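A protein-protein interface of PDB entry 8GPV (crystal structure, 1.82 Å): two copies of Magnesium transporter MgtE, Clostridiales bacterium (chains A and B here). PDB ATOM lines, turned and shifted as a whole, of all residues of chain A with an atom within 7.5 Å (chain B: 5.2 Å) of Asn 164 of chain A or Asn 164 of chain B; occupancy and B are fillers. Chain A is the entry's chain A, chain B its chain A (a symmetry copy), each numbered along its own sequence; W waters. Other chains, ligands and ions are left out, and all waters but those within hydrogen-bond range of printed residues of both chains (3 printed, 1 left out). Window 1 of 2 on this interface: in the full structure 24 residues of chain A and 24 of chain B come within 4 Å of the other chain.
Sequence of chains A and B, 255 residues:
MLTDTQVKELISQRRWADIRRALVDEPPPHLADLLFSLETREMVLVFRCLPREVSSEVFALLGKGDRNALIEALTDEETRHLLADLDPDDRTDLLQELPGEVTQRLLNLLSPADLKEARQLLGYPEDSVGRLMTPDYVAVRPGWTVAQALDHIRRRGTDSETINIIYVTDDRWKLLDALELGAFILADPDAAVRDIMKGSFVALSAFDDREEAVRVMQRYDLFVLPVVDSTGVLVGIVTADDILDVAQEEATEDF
Asn 164 of chain B touches just one residue of chain A: Asn 164.
Printed residues of chain B within 4 Å of Phe 223 of chain A: Phe 223.
Of the printed residues of chain B, Leu 181 of chain A touches Leu 181.
Of the printed residues of chain B, Gly 182 of chain A touches Ile 163.
Leu 179 of chain B touches none of the printed residues of chain A.
The nearest residue of chain A that does not touch Asn 164 of chain B is Phe 223 of chain A (4.5 Å).
The nearest printed residue of chain B that does not touch Leu 181 of chain A is Asn 164 of chain B (4.8 Å).
The side-chain amide nitrogen (ND2) of Asn 164 of chain A lies close to the side-chain amide nitrogen (ND2) of Asn 164 of chain B (3.5 Å).
Asn 164 of chain B touches its own counterpart, Asn 164 of chain A.
Leu 181 of chain A touches its own counterpart, Leu 181 of chain B.
Phe 223 of chain A touches its own counterpart, Phe 223 of chain B.
9 positions are printed for both chains.
Of the 4 pairs that touch across the chains among the printed residues, 3 have their exchanged pair printed and touching as well.
Leu 181 of chain B touches Leu 181 of chain A (CD2 to CD2, 3.8 Å).
CA of Gly 182 of chain A touches CD1 of Ile 163 of chain B, at 3.8 Å.
Phe 223 of chain A touches Phe 223 of chain B.
Of the 18 printed residues of chain A, 4 touch a printed residue of chain B.
Printed residues of chain A that touch a printed residue of chain B: Asn 164, Leu 181, Gly 182 and Phe 223.
Hydrophobic or aromatic side chains of chain A within 4 Å of the printed part of chain B: Leu 181 and Phe 223.
Printed residues of chain B that touch a printed residue of chain A: Ile 163, Asn 164, Leu 181 and Phe 223.
Hydrophobic or aromatic side chains of chain B that line the printed part of chain A: Ile 163, Leu 181 and Phe 223.
Among the printed residues, 4 pairs touch across the chains.
Among the printed residues, no Asp or Glu carboxylate lies within 4 Å of a Lys or Arg side-chain nitrogen of the other chain.
Water W1 lies within hydrogen-bond range of O of Asn 164 of chain A (2.7 Å) and OD1 of Asn 164 of chain B (2.9 Å).
Water W2 lies within hydrogen-bond range of O of Asn 164 of chain B (2.7 Å) and OD1 of Asn 164 of chain A (2.9 Å).
Water W3 bridges the side-chain amide nitrogen of Asn 164 of chain A and the backbone NH of Leu 181 of chain B.
O of Asn 164 of chain A lies within hydrogen-bond range of N of Leu 181 of chain A (3.0 Å).
The side-chain hydroxyl (OG1) of Thr 162 of chain A sits at hydrogen-bond distance from the backbone NH (N) of Asn 164 of chain A.
O of Asn 164 of chain B lies within hydrogen-bond range of N of Leu 181 of chain B.
The backbone NH (N) of Asn 164 of chain B lies within hydrogen-bond range of the side-chain hydroxyl (OG1) of Thr 162 of chain B, 3.1 Å away.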
ATOM      1  N   VAL A 138      -7.919  -3.190  -8.555  1.00  0.00           N
ATOM      2  CA  VAL A 138      -7.171  -3.665  -7.397  1.00  0.00           C
ATOM      3  C   VAL A 138      -8.097  -4.535  -6.571  1.00  0.00           C
ATOM      4  O   VAL A 138      -9.201  -4.107  -6.210  1.00  0.00           O
ATOM      5  CB  VAL A 138      -6.599  -2.502  -6.560  1.00  0.00           C
ATOM      6  CG1 VAL A 138      -5.897  -3.047  -5.346  1.00  0.00           C
ATOM      7  CG2 VAL A 138      -5.645  -1.635  -7.404  1.00  0.00           C
ATOM      8  N   ILE A 153      -2.594  -2.368  -1.741  1.00  0.00           N
ATOM      9  CA  ILE A 153      -3.060  -1.180  -2.439  1.00  0.00           C
ATOM     10  C   ILE A 153      -1.899  -0.231  -2.720  1.00  0.00           C
ATOM     11  O   ILE A 153      -1.851   0.421  -3.769  1.00  0.00           O
ATOM     12  CB  ILE A 153      -4.178  -0.502  -1.621  1.00  0.00           C
ATOM     13  CG1 ILE A 153      -5.420  -1.379  -1.632  1.00  0.00           C
ATOM     14  CG2 ILE A 153      -4.486   0.879  -2.183  1.00  0.00           C
ATOM     15  CD1 ILE A 153      -6.373  -1.198  -0.370  1.00  0.00           C
ATOM     16  N   SER A 160      -2.674   1.023 -11.632  1.00  0.00           N
ATOM     17  CA  SER A 160      -4.054   0.574 -11.746  1.00  0.00           C
ATOM     18  C   SER A 160      -4.975   1.739 -12.091  1.00  0.00           C
ATOM     19  O   SER A 160      -4.631   2.917 -11.908  1.00  0.00           O
ATOM     20  CB  SER A 160      -4.496  -0.093 -10.446  1.00  0.00           C
ATOM     21  OG  SER A 160      -4.680   0.898  -9.455  1.00  0.00           O
ATOM     22  N   GLU A 161      -6.165   1.400 -12.607  1.00  0.00           N
ATOM     23  CA  GLU A 161      -7.071   2.430 -13.111  1.00  0.00           C
ATOM     24  C   GLU A 161      -7.552   3.343 -11.990  1.00  0.00           C
ATOM     25  O   GLU A 161      -7.621   4.567 -12.155  1.00  0.00           O
ATOM     26  CB  GLU A 161      -8.284   1.783 -13.783  1.00  0.00           C
ATOM     27  CG  GLU A 161      -9.371   2.799 -14.208  1.00  0.00           C
ATOM     28  CD  GLU A 161      -8.924   3.695 -15.353  1.00  0.00           C
ATOM     29  OE1 GLU A 161      -8.134   3.231 -16.193  1.00  0.00           O
ATOM     30  OE2 GLU A 161      -9.366   4.864 -15.431  1.00  0.00           O
ATOM     31  N   THR A 162      -7.917   2.760 -10.860  1.00  0.00           N
ATOM     32  CA  THR A 162      -8.366   3.531  -9.711  1.00  0.00           C
ATOM     33  C   THR A 162      -8.205   2.666  -8.475  1.00  0.00           C
ATOM     34  O   THR A 162      -8.232   1.428  -8.558  1.00  0.00           O
ATOM     35  CB  THR A 162      -9.815   3.994  -9.885  1.00  0.00           C
ATOM     36  OG1 THR A 162     -10.198   4.810  -8.759  1.00  0.00           O
ATOM     37  CG2 THR A 162     -10.741   2.789  -9.991  1.00  0.00           C
ATOM     38  N   ILE A 163      -8.011   3.324  -7.328  1.00  0.00           N
ATOM     39  CA  ILE A 163      -8.041   2.633  -6.050  1.00  0.00           C
ATOM     40  C   ILE A 163      -9.177   3.123  -5.180  1.00  0.00           C
ATOM     41  O   ILE A 163      -9.239   2.794  -3.999  1.00  0.00           O
ATOM     42  CB  ILE A 163      -6.705   2.734  -5.290  1.00  0.00           C
ATOM     43  CG1 ILE A 163      -6.211   4.177  -5.167  1.00  0.00           C
ATOM     44  CG2 ILE A 163      -5.659   1.805  -5.938  1.00  0.00           C
ATOM     45  CD1 ILE A 163      -5.027   4.340  -4.177  1.00  0.00           C
ATOM     46  N   ASN A 164     -10.093   3.886  -5.753  1.00  0.00           N
ATOM     47  CA  ASN A 164     -11.159   4.459  -4.936  1.00  0.00           C
ATOM     48  C   ASN A 164     -12.204   3.430  -4.517  1.00  0.00           C
ATOM     49  O   ASN A 164     -12.840   3.590  -3.467  1.00  0.00           O
ATOM     50  CB  ASN A 164     -11.746   5.631  -5.687  1.00  0.00           C
ATOM     51  CG  ASN A 164     -10.834   6.839  -5.633  1.00  0.00           C
ATOM     52  OD1 ASN A 164     -10.866   7.708  -6.508  1.00  0.00           O
ATOM     53  ND2 ASN A 164     -10.004   6.903  -4.579  1.00  0.00           N
ATOM     54  N   ILE A 165     -12.374   2.360  -5.285  1.00  0.00           N
ATOM     55  CA  ILE A 165     -13.073   1.162  -4.838  1.00  0.00           C
ATOM     56  C   ILE A 165     -12.102   0.000  -4.968  1.00  0.00           C
ATOM     57  O   ILE A 165     -11.396  -0.124  -5.979  1.00  0.00           O
ATOM     58  CB  ILE A 165     -14.381   0.903  -5.625  1.00  0.00           C
ATOM     59  CG1 ILE A 165     -15.375   2.045  -5.397  1.00  0.00           C
ATOM     60  CG2 ILE A 165     -15.024  -0.448  -5.256  1.00  0.00           C
ATOM     61  CD1 ILE A 165     -16.093   1.998  -4.076  1.00  0.00           C
ATOM     62  N   ILE A 166     -12.068  -0.843  -3.938  1.00  0.00           N
ATOM     63  CA  ILE A 166     -11.228  -2.037  -3.876  1.00  0.00           C
ATOM     64  C   ILE A 166     -12.137  -3.259  -3.872  1.00  0.00           C
ATOM     65  O   ILE A 166     -13.095  -3.333  -3.089  1.00  0.00           O
ATOM     66  CB  ILE A 166     -10.317  -2.006  -2.634  1.00  0.00           C
ATOM     67  CG1 ILE A 166      -9.487  -0.711  -2.578  1.00  0.00           C
ATOM     68  CG2 ILE A 166      -9.449  -3.269  -2.549  1.00  0.00           C
ATOM     69  CD1 ILE A 166      -8.445  -0.554  -3.706  1.00  0.00           C
ATOM     70  N   TYR A 167     -11.868  -4.214  -4.760  1.00  0.00           N
ATOM     71  CA  TYR A 167     -12.731  -5.380  -4.875  1.00  0.00           C
ATOM     72  C   TYR A 167     -12.183  -6.521  -4.032  1.00  0.00           C
ATOM     73  O   TYR A 167     -10.978  -6.634  -3.813  1.00  0.00           O
ATOM     74  CB  TYR A 167     -12.900  -5.777  -6.357  1.00  0.00           C
ATOM     75  CG  TYR A 167     -13.579  -4.614  -7.039  1.00  0.00           C
ATOM     76  CD1 TYR A 167     -14.958  -4.432  -6.917  1.00  0.00           C
ATOM     77  CD2 TYR A 167     -12.834  -3.617  -7.682  1.00  0.00           C
ATOM     78  CE1 TYR A 167     -15.593  -3.340  -7.473  1.00  0.00           C
ATOM     79  CE2 TYR A 167     -13.471  -2.503  -8.244  1.00  0.00           C
ATOM     80  CZ  TYR A 167     -14.851  -2.372  -8.128  1.00  0.00           C
ATOM     81  OH  TYR A 167     -15.524  -1.275  -8.654  1.00  0.00           O
ATOM     82  N   LEU A 179     -15.506  -2.405  -1.819  1.00  0.00           N
ATOM     83  CA  LEU A 179     -15.288  -1.562  -0.651  1.00  0.00           C
ATOM     84  C   LEU A 179     -14.672  -0.226  -1.041  1.00  0.00           C
ATOM     85  O   LEU A 179     -13.773  -0.160  -1.888  1.00  0.00           O
ATOM     86  CB  LEU A 179     -14.383  -2.263   0.357  1.00  0.00           C
ATOM     87  CG  LEU A 179     -14.917  -3.579   0.922  1.00  0.00           C
ATOM     88  CD1 LEU A 179     -13.862  -4.225   1.784  1.00  0.00           C
ATOM     89  CD2 LEU A 179     -16.217  -3.359   1.701  1.00  0.00           C
ATOM     90  N   GLU A 180     -15.148   0.839  -0.405  1.00  0.00           N
ATOM     91  CA  GLU A 180     -14.538   2.142  -0.585  1.00  0.00           C
ATOM     92  C   GLU A 180     -13.135   2.138   0.015  1.00  0.00           C
ATOM     93  O   GLU A 180     -12.873   1.476   1.025  1.00  0.00           O
ATOM     94  CB  GLU A 180     -15.385   3.226   0.090  1.00  0.00           C
ATOM     95  CG  GLU A 180     -16.865   3.227  -0.301  1.00  0.00           C
ATOM     96  CD  GLU A 180     -17.655   4.313   0.430  1.00  0.00           C
ATOM     97  OE1 GLU A 180     -17.160   4.809   1.464  1.00  0.00           O
ATOM     98  OE2 GLU A 180     -18.753   4.678  -0.038  1.00  0.00           O
ATOM     99  N   LEU A 181     -12.229   2.884  -0.611  1.00  0.00           N
ATOM    100  CA  LEU A 181     -10.890   3.025  -0.046  1.00  0.00           C
ATOM    101  C   LEU A 181     -10.952   3.559   1.383  1.00  0.00           C
ATOM    102  O   LEU A 181     -10.195   3.111   2.254  1.00  0.00           O
ATOM    103  CB  LEU A 181     -10.041   3.933  -0.925  1.00  0.00           C
ATOM    104  CG  LEU A 181      -8.564   4.095  -0.538  1.00  0.00           C
ATOM    105  CD1 LEU A 181      -7.803   2.778  -0.678  1.00  0.00           C
ATOM    106  CD2 LEU A 181      -7.903   5.188  -1.382  1.00  0.00           C
ATOM    107  N   GLY A 182     -11.870   4.503   1.638  1.00  0.00           N
ATOM    108  CA  GLY A 182     -12.005   5.068   2.972  1.00  0.00           C
ATOM    109  C   GLY A 182     -12.238   4.040   4.059  1.00  0.00           C
ATOM    110  O   GLY A 182     -11.773   4.214   5.194  1.00  0.00           O
ATOM    111  N   ALA A 183     -12.972   2.971   3.743  1.00  0.00           N
ATOM    112  CA  ALA A 183     -13.238   1.935   4.734  1.00  0.00           C
ATOM    113  C   ALA A 183     -11.948   1.339   5.282  1.00  0.00           C
ATOM    114  O   ALA A 183     -11.880   0.982   6.466  1.00  0.00           O
ATOM    115  CB  ALA A 183     -14.114   0.840   4.133  1.00  0.00           C
ATOM    116  N   PHE A 184     -10.915   1.219   4.439  1.00  0.00           N
ATOM    117  CA  PHE A 184      -9.647   0.653   4.893  1.00  0.00           C
ATOM    118  C   PHE A 184      -8.872   1.605   5.805  1.00  0.00           C
ATOM    119  O   PHE A 184      -8.131   1.144   6.681  1.00  0.00           O
ATOM    120  CB  PHE A 184      -8.766   0.268   3.703  1.00  0.00           C
ATOM    121  CG  PHE A 184      -9.336  -0.825   2.839  1.00  0.00           C
ATOM    122  CD1 PHE A 184      -8.963  -2.147   3.038  1.00  0.00           C
ATOM    123  CD2 PHE A 184     -10.228  -0.531   1.825  1.00  0.00           C
ATOM    124  CE1 PHE A 184      -9.485  -3.158   2.247  1.00  0.00           C
ATOM    125  CE2 PHE A 184     -10.752  -1.533   1.025  1.00  0.00           C
ATOM    126  CZ  PHE A 184     -10.385  -2.851   1.234  1.00  0.00           C
ATOM    127  N   PHE A 223     -18.917   5.635  -8.847  1.00  0.00           N
ATOM    128  CA  PHE A 223     -17.959   6.113  -9.851  1.00  0.00           C
ATOM    129  C   PHE A 223     -17.239   4.978 -10.576  1.00  0.00           C
ATOM    130  O   PHE A 223     -16.550   5.241 -11.569  1.00  0.00           O
ATOM    131  CB  PHE A 223     -16.894   7.017  -9.222  1.00  0.00           C
ATOM    132  CG  PHE A 223     -17.448   8.198  -8.492  1.00  0.00           C
ATOM    133  CD1 PHE A 223     -18.668   8.746  -8.857  1.00  0.00           C
ATOM    134  CD2 PHE A 223     -16.740   8.770  -7.445  1.00  0.00           C
ATOM    135  CE1 PHE A 223     -19.191   9.837  -8.174  1.00  0.00           C
ATOM    136  CE2 PHE A 223     -17.255   9.871  -6.760  1.00  0.00           C
ATOM    137  CZ  PHE A 223     -18.476  10.400  -7.132  1.00  0.00           C
ATOM    138  N   VAL A 224     -17.334   3.745 -10.081  1.00  0.00           N
ATOM    139  CA  VAL A 224     -16.723   2.576 -10.722  1.00  0.00           C
ATOM    140  C   VAL A 224     -17.673   1.396 -10.553  1.00  0.00           C
ATOM    141  O   VAL A 224     -18.361   1.274  -9.536  1.00  0.00           O
ATOM    142  CB  VAL A 224     -15.323   2.277 -10.119  1.00  0.00           C
ATOM    143  CG1 VAL A 224     -15.456   2.003  -8.703  1.00  0.00           C
ATOM    144  CG2 VAL A 224     -14.599   1.064 -10.801  1.00  0.00           C
ATOM    145  N   THR B 162     -17.889  13.098  -0.243  1.00  0.00           N
ATOM    146  CA  THR B 162     -16.892  12.140  -0.695  1.00  0.00           C
ATOM    147  C   THR B 162     -15.569  12.500  -0.045  1.00  0.00           C
ATOM    148  O   THR B 162     -15.331  13.666   0.307  1.00  0.00           O
ATOM    149  CB  THR B 162     -16.781  12.133  -2.222  1.00  0.00           C
ATOM    150  OG1 THR B 162     -15.835  11.125  -2.631  1.00  0.00           O
ATOM    151  CG2 THR B 162     -16.332  13.500  -2.722  1.00  0.00           C
ATOM    152  N   ILE B 163     -14.717  11.486   0.136  1.00  0.00           N
ATOM    153  CA  ILE B 163     -13.348  11.721   0.561  1.00  0.00           C
ATOM    154  C   ILE B 163     -12.356  11.280  -0.494  1.00  0.00           C
ATOM    155  O   ILE B 163     -11.158  11.223  -0.231  1.00  0.00           O
ATOM    156  CB  ILE B 163     -13.023  11.055   1.911  1.00  0.00           C
ATOM    157  CG1 ILE B 163     -13.400   9.572   1.936  1.00  0.00           C
ATOM    158  CG2 ILE B 163     -13.674  11.849   3.060  1.00  0.00           C
ATOM    159  CD1 ILE B 163     -12.836   8.814   3.168  1.00  0.00           C
ATOM    160  N   ASN B 164     -12.835  10.992  -1.692  1.00  0.00           N
ATOM    161  CA  ASN B 164     -11.932  10.474  -2.717  1.00  0.00           C
ATOM    162  C   ASN B 164     -11.006  11.544  -3.287  1.00  0.00           C
ATOM    163  O   ASN B 164      -9.898  11.223  -3.737  1.00  0.00           O
ATOM    164  CB  ASN B 164     -12.766   9.786  -3.771  1.00  0.00           C
ATOM    165  CG  ASN B 164     -13.261   8.436  -3.295  1.00  0.00           C
ATOM    166  OD1 ASN B 164     -14.283   7.926  -3.760  1.00  0.00           O
ATOM    167  ND2 ASN B 164     -12.518   7.837  -2.350  1.00  0.00           N
ATOM    168  N   ILE B 165     -11.408  12.809  -3.246  1.00  0.00           N
ATOM    169  CA  ILE B 165     -10.507  13.938  -3.435  1.00  0.00           C
ATOM    170  C   ILE B 165     -10.598  14.800  -2.187  1.00  0.00           C
ATOM    171  O   ILE B 165     -11.697  15.058  -1.676  1.00  0.00           O
ATOM    172  CB  ILE B 165     -10.825  14.751  -4.715  1.00  0.00           C
ATOM    173  CG1 ILE B 165     -10.631  13.881  -5.960  1.00  0.00           C
ATOM    174  CG2 ILE B 165      -9.972  16.030  -4.818  1.00  0.00           C
ATOM    175  CD1 ILE B 165      -9.197  13.684  -6.372  1.00  0.00           C
ATOM    176  N   ILE B 166      -9.438  15.236  -1.700  1.00  0.00           N
ATOM    177  CA  ILE B 166      -9.307  16.100  -0.529  1.00  0.00           C
ATOM    178  C   ILE B 166      -8.755  17.444  -0.987  1.00  0.00           C
ATOM    179  O   ILE B 166      -7.752  17.503  -1.713  1.00  0.00           O
ATOM    180  CB  ILE B 166      -8.403  15.452   0.536  1.00  0.00           C
ATOM    181  CG1 ILE B 166      -8.896  14.041   0.908  1.00  0.00           C
ATOM    182  CG2 ILE B 166      -8.240  16.364   1.759  1.00  0.00           C
ATOM    183  CD1 ILE B 166     -10.263  13.996   1.623  1.00  0.00           C
ATOM    184  N   LEU B 179      -6.156  16.852  -4.018  1.00  0.00           N
ATOM    185  CA  LEU B 179      -5.338  15.656  -3.869  1.00  0.00           C
ATOM    186  C   LEU B 179      -6.199  14.404  -3.790  1.00  0.00           C
ATOM    187  O   LEU B 179      -7.244  14.387  -3.129  1.00  0.00           O
ATOM    188  CB  LEU B 179      -4.467  15.753  -2.621  1.00  0.00           C
ATOM    189  CG  LEU B 179      -3.470  16.912  -2.598  1.00  0.00           C
ATOM    190  CD1 LEU B 179      -2.790  16.966  -1.254  1.00  0.00           C
ATOM    191  CD2 LEU B 179      -2.452  16.787  -3.735  1.00  0.00           C
ATOM    192  N   GLU B 180      -5.745  13.346  -4.455  1.00  0.00           N
ATOM    193  CA  GLU B 180      -6.400  12.059  -4.332  1.00  0.00           C
ATOM    194  C   GLU B 180      -6.216  11.522  -2.916  1.00  0.00           C
ATOM    195  O   GLU B 180      -5.181  11.743  -2.278  1.00  0.00           O
ATOM    196  CB  GLU B 180      -5.816  11.064  -5.341  1.00  0.00           C
ATOM    197  CG  GLU B 180      -5.785  11.556  -6.791  1.00  0.00           C
ATOM    198  CD  GLU B 180      -5.163  10.528  -7.736  1.00  0.00           C
ATOM    199  OE1 GLU B 180      -4.457   9.623  -7.244  1.00  0.00           O
ATOM    200  OE2 GLU B 180      -5.396  10.615  -8.960  1.00  0.00           O
ATOM    201  N   LEU B 181      -7.228  10.812  -2.424  1.00  0.00           N
ATOM    202  CA  LEU B 181      -7.095  10.170  -1.118  1.00  0.00           C
ATOM    203  C   LEU B 181      -5.882   9.244  -1.085  1.00  0.00           C
ATOM    204  O   LEU B 181      -5.161   9.190  -0.079  1.00  0.00           O
ATOM    205  CB  LEU B 181      -8.366   9.406  -0.777  1.00  0.00           C
ATOM    206  CG  LEU B 181      -8.442   8.767   0.617  1.00  0.00           C
ATOM    207  CD1 LEU B 181      -8.448   9.827   1.717  1.00  0.00           C
ATOM    208  CD2 LEU B 181      -9.677   7.869   0.732  1.00  0.00           C
ATOM    209  N   PHE B 223     -13.790  12.571 -11.024  1.00  0.00           N
ATOM    210  CA  PHE B 223     -15.100  12.213 -10.467  1.00  0.00           C
ATOM    211  C   PHE B 223     -15.684  13.302  -9.570  1.00  0.00           C
ATOM    212  O   PHE B 223     -16.859  13.204  -9.193  1.00  0.00           O
ATOM    213  CB  PHE B 223     -15.025  10.921  -9.647  1.00  0.00           C
ATOM    214  CG  PHE B 223     -14.491   9.748 -10.404  1.00  0.00           C
ATOM    215  CD1 PHE B 223     -14.642   9.665 -11.779  1.00  0.00           C
ATOM    216  CD2 PHE B 223     -13.849   8.715  -9.735  1.00  0.00           C
ATOM    217  CE1 PHE B 223     -14.137   8.581 -12.488  1.00  0.00           C
ATOM    218  CE2 PHE B 223     -13.348   7.619 -10.438  1.00  0.00           C
ATOM    219  CZ  PHE B 223     -13.499   7.558 -11.810  1.00  0.00           C
HETATM  220  O   HOH W   1     -14.707   5.293  -2.610  1.00  0.00           O
HETATM  221  O   HOH W   2      -9.026   9.859  -5.858  1.00  0.00           O
HETATM  222  O   HOH W   3      -7.302   7.987  -4.232  1.00  0.00           O
